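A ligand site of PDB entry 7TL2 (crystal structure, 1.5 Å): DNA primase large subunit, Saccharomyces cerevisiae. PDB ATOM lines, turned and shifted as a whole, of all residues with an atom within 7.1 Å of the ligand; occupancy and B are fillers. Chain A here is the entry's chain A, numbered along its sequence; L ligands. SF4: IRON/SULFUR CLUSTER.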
ATOM      1  N   PRO A  23      35.217 -22.469  -8.758  1.00  0.00           N
ATOM      2  CA  PRO A  23      34.359 -22.556  -7.550  1.00  0.00           C
ATOM      3  C   PRO A  23      33.499 -23.803  -7.634  1.00  0.00           C
ATOM      4  O   PRO A  23      33.392 -24.445  -8.688  1.00  0.00           O
ATOM      5  CB  PRO A  23      33.500 -21.267  -7.603  1.00  0.00           C
ATOM      6  CG  PRO A  23      33.437 -20.916  -9.075  1.00  0.00           C
ATOM      7  CD  PRO A  23      34.793 -21.377  -9.673  1.00  0.00           C
ATOM      8  N   LEU A  24      32.808 -24.111  -6.525  1.00  0.00           N
ATOM      9  CA  LEU A  24      32.075 -25.375  -6.470  1.00  0.00           C
ATOM     10  C   LEU A  24      30.996 -25.479  -7.540  1.00  0.00           C
ATOM     11  O   LEU A  24      30.742 -26.568  -8.060  1.00  0.00           O
ATOM     12  CB  LEU A  24      31.431 -25.593  -5.083  1.00  0.00           C
ATOM     13  CG  LEU A  24      32.382 -25.895  -3.938  1.00  0.00           C
ATOM     14  CD1 LEU A  24      31.640 -26.547  -2.807  1.00  0.00           C
ATOM     15  CD2 LEU A  24      33.493 -26.837  -4.460  1.00  0.00           C
ATOM     16  N   CYS A  25      30.286 -24.380  -7.873  1.00  0.00           N
ATOM     17  CA  CYS A  25      29.235 -24.497  -8.903  1.00  0.00           C
ATOM     18  C   CYS A  25      29.811 -24.963 -10.224  1.00  0.00           C
ATOM     19  O   CYS A  25      29.217 -25.813 -10.893  1.00  0.00           O
ATOM     20  CB  CYS A  25      28.456 -23.159  -9.067  1.00  0.00           C
ATOM     21  SG  CYS A  25      29.492 -21.739  -9.486  1.00  0.00           S
ATOM     22  N   ILE A  26      30.961 -24.397 -10.598  1.00  0.00           N
ATOM     23  CA  ILE A  26      31.570 -24.779 -11.870  1.00  0.00           C
ATOM     24  C   ILE A  26      32.110 -26.186 -11.794  1.00  0.00           C
ATOM     25  O   ILE A  26      31.993 -26.958 -12.757  1.00  0.00           O
ATOM     26  CB  ILE A  26      32.643 -23.770 -12.277  1.00  0.00           C
ATOM     27  CG1 ILE A  26      32.030 -22.371 -12.453  1.00  0.00           C
ATOM     28  CG2 ILE A  26      33.416 -24.224 -13.540  1.00  0.00           C
ATOM     29  CD1 ILE A  26      30.824 -22.263 -13.444  1.00  0.00           C
ATOM     30  N   GLN A  46      25.063 -21.465 -17.603  1.00  0.00           N
ATOM     31  CA  GLN A  46      25.969 -21.106 -16.513  1.00  0.00           C
ATOM     32  C   GLN A  46      27.403 -21.503 -16.831  1.00  0.00           C
ATOM     33  O   GLN A  46      28.332 -20.695 -16.665  1.00  0.00           O
ATOM     34  CB  GLN A  46      25.487 -21.799 -15.223  1.00  0.00           C
ATOM     35  CG  GLN A  46      26.283 -21.348 -13.953  1.00  0.00           C
ATOM     36  CD  GLN A  46      25.637 -21.856 -12.684  1.00  0.00           C
ATOM     37  OE1 GLN A  46      24.480 -22.187 -12.672  1.00  0.00           O
ATOM     38  NE2 GLN A  46      26.401 -21.885 -11.610  1.00  0.00           N
ATOM     39  N   ASP A 105      26.799 -13.626 -12.647  1.00  0.00           N
ATOM     40  CA  ASP A 105      27.281 -13.463 -11.282  1.00  0.00           C
ATOM     41  C   ASP A 105      26.495 -14.375 -10.328  1.00  0.00           C
ATOM     42  O   ASP A 105      25.543 -15.073 -10.705  1.00  0.00           O
ATOM     43  CB  ASP A 105      27.246 -11.993 -10.893  1.00  0.00           C
ATOM     44  CG  ASP A 105      25.837 -11.365 -10.896  1.00  0.00           C
ATOM     45  OD1 ASP A 105      24.803 -12.051 -10.902  1.00  0.00           O
ATOM     46  OD2 ASP A 105      25.793 -10.130 -10.865  1.00  0.00           O
ATOM     47  N   CYS A 106      26.890 -14.382  -9.042  1.00  0.00           N
ATOM     48  CA  CYS A 106      26.260 -15.273  -8.069  1.00  0.00           C
ATOM     49  C   CYS A 106      24.789 -14.925  -7.890  1.00  0.00           C
ATOM     50  O   CYS A 106      23.947 -15.808  -7.736  1.00  0.00           O
ATOM     51  CB  CYS A 106      27.019 -15.250  -6.706  1.00  0.00           C
ATOM     52  SG  CYS A 106      28.762 -15.792  -6.906  1.00  0.00           S
ATOM     53  N   HIS A 107      24.485 -13.626  -7.857  1.00  0.00           N
ATOM     54  CA  HIS A 107      23.090 -13.239  -7.709  1.00  0.00           C
ATOM     55  C   HIS A 107      22.235 -13.782  -8.858  1.00  0.00           C
ATOM     56  O   HIS A 107      21.138 -14.309  -8.615  1.00  0.00           O
ATOM     57  CB  HIS A 107      22.945 -11.716  -7.639  1.00  0.00           C
ATOM     58  CG  HIS A 107      21.526 -11.263  -7.621  1.00  0.00           C
ATOM     59  ND1 HIS A 107      20.707 -11.405  -6.513  1.00  0.00           N
ATOM     60  CD2 HIS A 107      20.730 -10.768  -8.608  1.00  0.00           C
ATOM     61  CE1 HIS A 107      19.501 -10.951  -6.797  1.00  0.00           C
ATOM     62  NE2 HIS A 107      19.493 -10.558  -8.060  1.00  0.00           N
ATOM     63  N   ILE A 109      22.956 -16.428 -10.783  1.00  0.00           N
ATOM     64  CA  ILE A 109      22.902 -17.879 -10.572  1.00  0.00           C
ATOM     65  C   ILE A 109      21.861 -18.257  -9.530  1.00  0.00           C
ATOM     66  O   ILE A 109      21.052 -19.183  -9.746  1.00  0.00           O
ATOM     67  CB  ILE A 109      24.319 -18.383 -10.210  1.00  0.00           C
ATOM     68  CG1 ILE A 109      25.217 -18.351 -11.447  1.00  0.00           C
ATOM     69  CG2 ILE A 109      24.295 -19.824  -9.668  1.00  0.00           C
ATOM     70  CD1 ILE A 109      26.672 -18.404 -11.129  1.00  0.00           C
ATOM     71  N   LEU A 110      21.911 -17.618  -8.345  1.00  0.00           N
ATOM     72  CA  LEU A 110      21.005 -17.951  -7.255  1.00  0.00           C
ATOM     73  C   LEU A 110      19.551 -17.630  -7.636  1.00  0.00           C
ATOM     74  O   LEU A 110      18.620 -18.273  -7.133  1.00  0.00           O
ATOM     75  CB  LEU A 110      21.437 -17.202  -5.975  1.00  0.00           C
ATOM     76  CG  LEU A 110      22.744 -17.748  -5.381  1.00  0.00           C
ATOM     77  CD1 LEU A 110      23.381 -16.660  -4.525  1.00  0.00           C
ATOM     78  CD2 LEU A 110      22.415 -18.997  -4.589  1.00  0.00           C
ATOM     79  N   GLY A 122      23.060 -23.717 -10.528  1.00  0.00           N
ATOM     80  CA  GLY A 122      22.775 -23.230  -9.180  1.00  0.00           C
ATOM     81  C   GLY A 122      24.053 -23.063  -8.371  1.00  0.00           C
ATOM     82  O   GLY A 122      25.145 -22.919  -8.911  1.00  0.00           O
ATOM     83  N   CYS A 123      23.889 -23.065  -7.040  1.00  0.00           N
ATOM     84  CA  CYS A 123      24.990 -22.851  -6.111  1.00  0.00           C
ATOM     85  C   CYS A 123      25.025 -24.025  -5.132  1.00  0.00           C
ATOM     86  O   CYS A 123      24.078 -24.172  -4.323  1.00  0.00           O
ATOM     87  CB  CYS A 123      24.791 -21.529  -5.369  1.00  0.00           C
ATOM     88  SG  CYS A 123      26.047 -21.278  -4.091  1.00  0.00           S
ATOM     89  N   PRO A 124      26.070 -24.860  -5.124  1.00  0.00           N
ATOM     90  CA  PRO A 124      26.104 -26.011  -4.195  1.00  0.00           C
ATOM     91  C   PRO A 124      25.985 -25.641  -2.747  1.00  0.00           C
ATOM     92  O   PRO A 124      25.440 -26.432  -1.966  1.00  0.00           O
ATOM     93  CB  PRO A 124      27.452 -26.668  -4.511  1.00  0.00           C
ATOM     94  CG  PRO A 124      27.598 -26.390  -6.055  1.00  0.00           C
ATOM     95  CD  PRO A 124      27.098 -24.970  -6.182  1.00  0.00           C
ATOM     96  N   PHE A 125      26.413 -24.452  -2.360  1.00  0.00           N
ATOM     97  CA  PHE A 125      26.315 -24.105  -0.941  1.00  0.00           C
ATOM     98  C   PHE A 125      24.866 -24.001  -0.500  1.00  0.00           C
ATOM     99  O   PHE A 125      24.566 -24.204   0.694  1.00  0.00           O
ATOM    100  CB  PHE A 125      27.079 -22.807  -0.668  1.00  0.00           C
ATOM    101  CG  PHE A 125      28.560 -22.958  -0.909  1.00  0.00           C
ATOM    102  CD1 PHE A 125      29.350 -23.641   0.030  1.00  0.00           C
ATOM    103  CD2 PHE A 125      29.131 -22.466  -2.077  1.00  0.00           C
ATOM    104  CE1 PHE A 125      30.720 -23.859  -0.200  1.00  0.00           C
ATOM    105  CE2 PHE A 125      30.519 -22.648  -2.287  1.00  0.00           C
ATOM    106  CZ  PHE A 125      31.304 -23.362  -1.348  1.00  0.00           C
ATOM    107  N   ARG A 126      23.940 -23.675  -1.425  1.00  0.00           N
ATOM    108  CA  ARG A 126      22.511 -23.685  -1.163  1.00  0.00           C
ATOM    109  C   ARG A 126      21.894 -25.024  -1.498  1.00  0.00           C
ATOM    110  O   ARG A 126      20.993 -25.477  -0.777  1.00  0.00           O
ATOM    111  CB  ARG A 126      21.846 -22.582  -1.996  1.00  0.00           C
ATOM    112  CG  ARG A 126      20.318 -22.542  -1.814  1.00  0.00           C
ATOM    113  CD  ARG A 126      19.650 -21.619  -2.846  1.00  0.00           C
ATOM    114  NE  ARG A 126      19.836 -22.190  -4.163  1.00  0.00           N
ATOM    115  CZ  ARG A 126      19.558 -21.580  -5.315  1.00  0.00           C
ATOM    116  NH1 ARG A 126      19.076 -20.323  -5.281  1.00  0.00           N
ATOM    117  NH2 ARG A 126      19.817 -22.252  -6.442  1.00  0.00           N
ATOM    118  N   TYR A 159      25.387 -17.838   1.198  1.00  0.00           N
ATOM    119  CA  TYR A 159      26.084 -18.776   0.300  1.00  0.00           C
ATOM    120  C   TYR A 159      27.363 -18.177  -0.266  1.00  0.00           C
ATOM    121  O   TYR A 159      28.358 -18.887  -0.378  1.00  0.00           O
ATOM    122  CB  TYR A 159      25.150 -19.189  -0.850  1.00  0.00           C
ATOM    123  CG  TYR A 159      23.863 -19.672  -0.275  1.00  0.00           C
ATOM    124  CD1 TYR A 159      23.835 -20.747   0.613  1.00  0.00           C
ATOM    125  CD2 TYR A 159      22.666 -19.044  -0.620  1.00  0.00           C
ATOM    126  CE1 TYR A 159      22.616 -21.162   1.237  1.00  0.00           C
ATOM    127  CE2 TYR A 159      21.483 -19.455  -0.037  1.00  0.00           C
ATOM    128  CZ  TYR A 159      21.451 -20.517   0.881  1.00  0.00           C
ATOM    129  OH  TYR A 159      20.231 -20.933   1.444  1.00  0.00           O
ATOM    130  N   THR A 160      27.361 -16.878  -0.586  1.00  0.00           N
ATOM    131  CA  THR A 160      28.608 -16.319  -1.130  1.00  0.00           C
ATOM    132  C   THR A 160      29.669 -16.162  -0.040  1.00  0.00           C
ATOM    133  O   THR A 160      30.870 -16.182  -0.370  1.00  0.00           O
ATOM    134  CB  THR A 160      28.362 -14.990  -1.829  1.00  0.00           C
ATOM    135  OG1 THR A 160      27.822 -14.030  -0.891  1.00  0.00           O
ATOM    136  CG2 THR A 160      27.323 -15.170  -2.949  1.00  0.00           C
ATOM    137  N   ILE A 161      29.292 -16.010   1.242  1.00  0.00           N
ATOM    138  CA  ILE A 161      30.289 -16.045   2.304  1.00  0.00           C
ATOM    139  C   ILE A 161      30.834 -17.443   2.490  1.00  0.00           C
ATOM    140  O   ILE A 161      32.042 -17.630   2.662  1.00  0.00           O
ATOM    141  CB  ILE A 161      29.700 -15.516   3.625  1.00  0.00           C
ATOM    142  CG1 ILE A 161      29.199 -14.097   3.418  1.00  0.00           C
ATOM    143  CG2 ILE A 161      30.718 -15.708   4.738  1.00  0.00           C
ATOM    144  CD1 ILE A 161      30.265 -13.104   3.262  1.00  0.00           C
ATOM    145  N   ALA A 162      29.976 -18.466   2.385  1.00  0.00           N
ATOM    146  CA  ALA A 162      30.476 -19.843   2.432  1.00  0.00           C
ATOM    147  C   ALA A 162      31.525 -20.087   1.345  1.00  0.00           C
ATOM    148  O   ALA A 162      32.569 -20.705   1.611  1.00  0.00           O
ATOM    149  CB  ALA A 162      29.318 -20.837   2.279  1.00  0.00           C
ATOM    150  N   CYS A 163      31.250 -19.625   0.123  1.00  0.00           N
ATOM    151  CA  CYS A 163      32.157 -19.797  -1.003  1.00  0.00           C
ATOM    152  C   CYS A 163      33.457 -19.031  -0.759  1.00  0.00           C
ATOM    153  O   CYS A 163      34.551 -19.547  -1.065  1.00  0.00           O
ATOM    154  CB  CYS A 163      31.417 -19.300  -2.241  1.00  0.00           C
ATOM    155  SG  CYS A 163      32.279 -19.578  -3.786  1.00  0.00           S
ATOM    156  N   THR A 164      33.350 -17.814  -0.218  1.00  0.00           N
ATOM    157  CA  THR A 164      34.566 -17.038   0.096  1.00  0.00           C
ATOM    158  C   THR A 164      35.405 -17.756   1.155  1.00  0.00           C
ATOM    159  O   THR A 164      36.643 -17.815   1.045  1.00  0.00           O
ATOM    160  CB  THR A 164      34.169 -15.640   0.609  1.00  0.00           C
ATOM    161  OG1 THR A 164      33.405 -14.971  -0.400  1.00  0.00           O
ATOM    162  CG2 THR A 164      35.412 -14.811   0.882  1.00  0.00           C
ATOM    163  N   ALA A 187      30.222 -10.576  -5.928  1.00  0.00           N
ATOM    164  CA  ALA A 187      30.167 -12.029  -5.836  1.00  0.00           C
ATOM    165  C   ALA A 187      30.022 -12.566  -7.251  1.00  0.00           C
ATOM    166  O   ALA A 187      28.994 -12.331  -7.905  1.00  0.00           O
ATOM    167  CB  ALA A 187      29.008 -12.505  -4.953  1.00  0.00           C
ATOM    168  N   HIS A 188      31.032 -13.333  -7.714  1.00  0.00           N
ATOM    169  CA  HIS A 188      31.035 -13.733  -9.121  1.00  0.00           C
ATOM    170  C   HIS A 188      31.942 -14.949  -9.299  1.00  0.00           C
ATOM    171  O   HIS A 188      33.112 -14.901  -8.939  1.00  0.00           O
ATOM    172  CB  HIS A 188      31.533 -12.572  -9.974  1.00  0.00           C
ATOM    173  CG  HIS A 188      31.172 -12.652 -11.430  1.00  0.00           C
ATOM    174  ND1 HIS A 188      31.555 -13.699 -12.265  1.00  0.00           N
ATOM    175  CD2 HIS A 188      30.479 -11.781 -12.211  1.00  0.00           C
ATOM    176  CE1 HIS A 188      31.087 -13.463 -13.483  1.00  0.00           C
ATOM    177  NE2 HIS A 188      30.447 -12.296 -13.477  1.00  0.00           N
ATOM    178  N   PRO A 189      31.445 -16.028  -9.917  1.00  0.00           N
ATOM    179  CA  PRO A 189      32.325 -17.186 -10.165  1.00  0.00           C
ATOM    180  C   PRO A 189      33.587 -16.839 -10.938  1.00  0.00           C
ATOM    181  O   PRO A 189      34.635 -17.471 -10.702  1.00  0.00           O
ATOM    182  CB  PRO A 189      31.412 -18.156 -10.960  1.00  0.00           C
ATOM    183  CG  PRO A 189      29.974 -17.722 -10.611  1.00  0.00           C
ATOM    184  CD  PRO A 189      30.067 -16.218 -10.424  1.00  0.00           C
ATOM    185  N   ASN A 190      33.488 -15.857 -11.865  1.00  0.00           N
ATOM    186  CA  ASN A 190      34.692 -15.536 -12.637  1.00  0.00           C
ATOM    187  C   ASN A 190      35.688 -14.777 -11.801  1.00  0.00           C
ATOM    188  O   ASN A 190      36.906 -14.873 -12.061  1.00  0.00           O
ATOM    189  CB  ASN A 190      34.334 -14.752 -13.900  1.00  0.00           C
ATOM    190  CG  ASN A 190      33.719 -15.663 -14.948  1.00  0.00           C
ATOM    191  OD1 ASN A 190      32.523 -15.963 -14.896  1.00  0.00           O
ATOM    192  ND2 ASN A 190      34.571 -16.209 -15.821  1.00  0.00           N
ATOM    193  N   TYR A 192      36.094 -15.528  -8.549  1.00  0.00           N
ATOM    194  CA  TYR A 192      36.735 -16.632  -7.845  1.00  0.00           C
ATOM    195  C   TYR A 192      37.860 -17.215  -8.690  1.00  0.00           C
ATOM    196  O   TYR A 192      38.976 -17.430  -8.218  1.00  0.00           O
ATOM    197  CB  TYR A 192      35.688 -17.700  -7.538  1.00  0.00           C
ATOM    198  CG  TYR A 192      36.117 -18.805  -6.593  1.00  0.00           C
ATOM    199  CD1 TYR A 192      37.041 -19.785  -6.964  1.00  0.00           C
ATOM    200  CD2 TYR A 192      35.495 -18.934  -5.357  1.00  0.00           C
ATOM    201  CE1 TYR A 192      37.371 -20.841  -6.068  1.00  0.00           C
ATOM    202  CE2 TYR A 192      35.781 -19.945  -4.492  1.00  0.00           C
ATOM    203  CZ  TYR A 192      36.719 -20.876  -4.822  1.00  0.00           C
ATOM    204  OH  TYR A 192      36.978 -21.895  -3.937  1.00  0.00           O
HETATM  205 FE1  SF4 L   1      29.289 -20.435  -7.575  1.00  0.00          FE
HETATM  206 FE2  SF4 L   1      28.740 -18.020  -6.449  1.00  0.00          FE
HETATM  207 FE3  SF4 L   1      30.463 -19.737  -5.220  1.00  0.00          FE
HETATM  208 FE4  SF4 L   1      27.815 -20.308  -5.283  1.00  0.00          FE
HETATM  209  S1  SF4 L   1      28.754 -18.562  -4.234  1.00  0.00           S
HETATM  210  S2  SF4 L   1      29.577 -21.737  -5.717  1.00  0.00           S
HETATM  211  S3  SF4 L   1      27.237 -19.465  -7.305  1.00  0.00           S
HETATM  212  S4  SF4 L   1      30.771 -18.807  -7.269  1.00  0.00           S
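N of Cys 25 lies close to S2 of the ligand (3.5 Å).
An iron atom (FE4) of the ligand is bound by the side-chain sulfur (SG) of Cys 123 (2.3 Å).
SG of Cys 25 is bound to FE1 of the ligand, 2.3 Å away.
SG of Cys 163 binds FE3 of the ligand (2.3 Å).
FE2 of the ligand is bound by SG of Cys 106, 2.3 Å away.
SG of Cys 106 sits close to N of His 188 (3.4 Å).
OG1 of Thr 164 lies within hydrogen-bond range of O of Thr 160, 2.8 Å away.
The backbone carbonyl oxygen of Ala 187 sits at hydrogen-bond distance from the backbone NH of Cys 106 (3.2 Å).
The side-chain sulfur (SG) of Cys 123 sits close to the backbone NH (N) of Phe 125 (3.6 Å).
The side-chain sulfur (SG) of Cys 25 lies close to the side-chain amide nitrogen (NE2) of Gln 46.
Pro 23 touches the ligand.
CG2 of Ile 109 touches S3 of the ligand, at 3.8 Å.
CE2 of Phe 125 touches S2 of the ligand, 3.7 Å away.
Tyr 159 touches the ligand (O to S1, 3.9 Å).
CA of Thr 160 touches S1 of the ligand, 3.8 Å away.
Pro 189 touches the ligand.
Within 4 Å of the ligand: Pro 23, Cys 25, Cys 106, Ile 109, Cys 123, Phe 125, Tyr 159, Thr 160, Cys 163 and Pro 189.
The nearest printed residue that does not touch the ligand is Leu 24 (4.1 Å).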
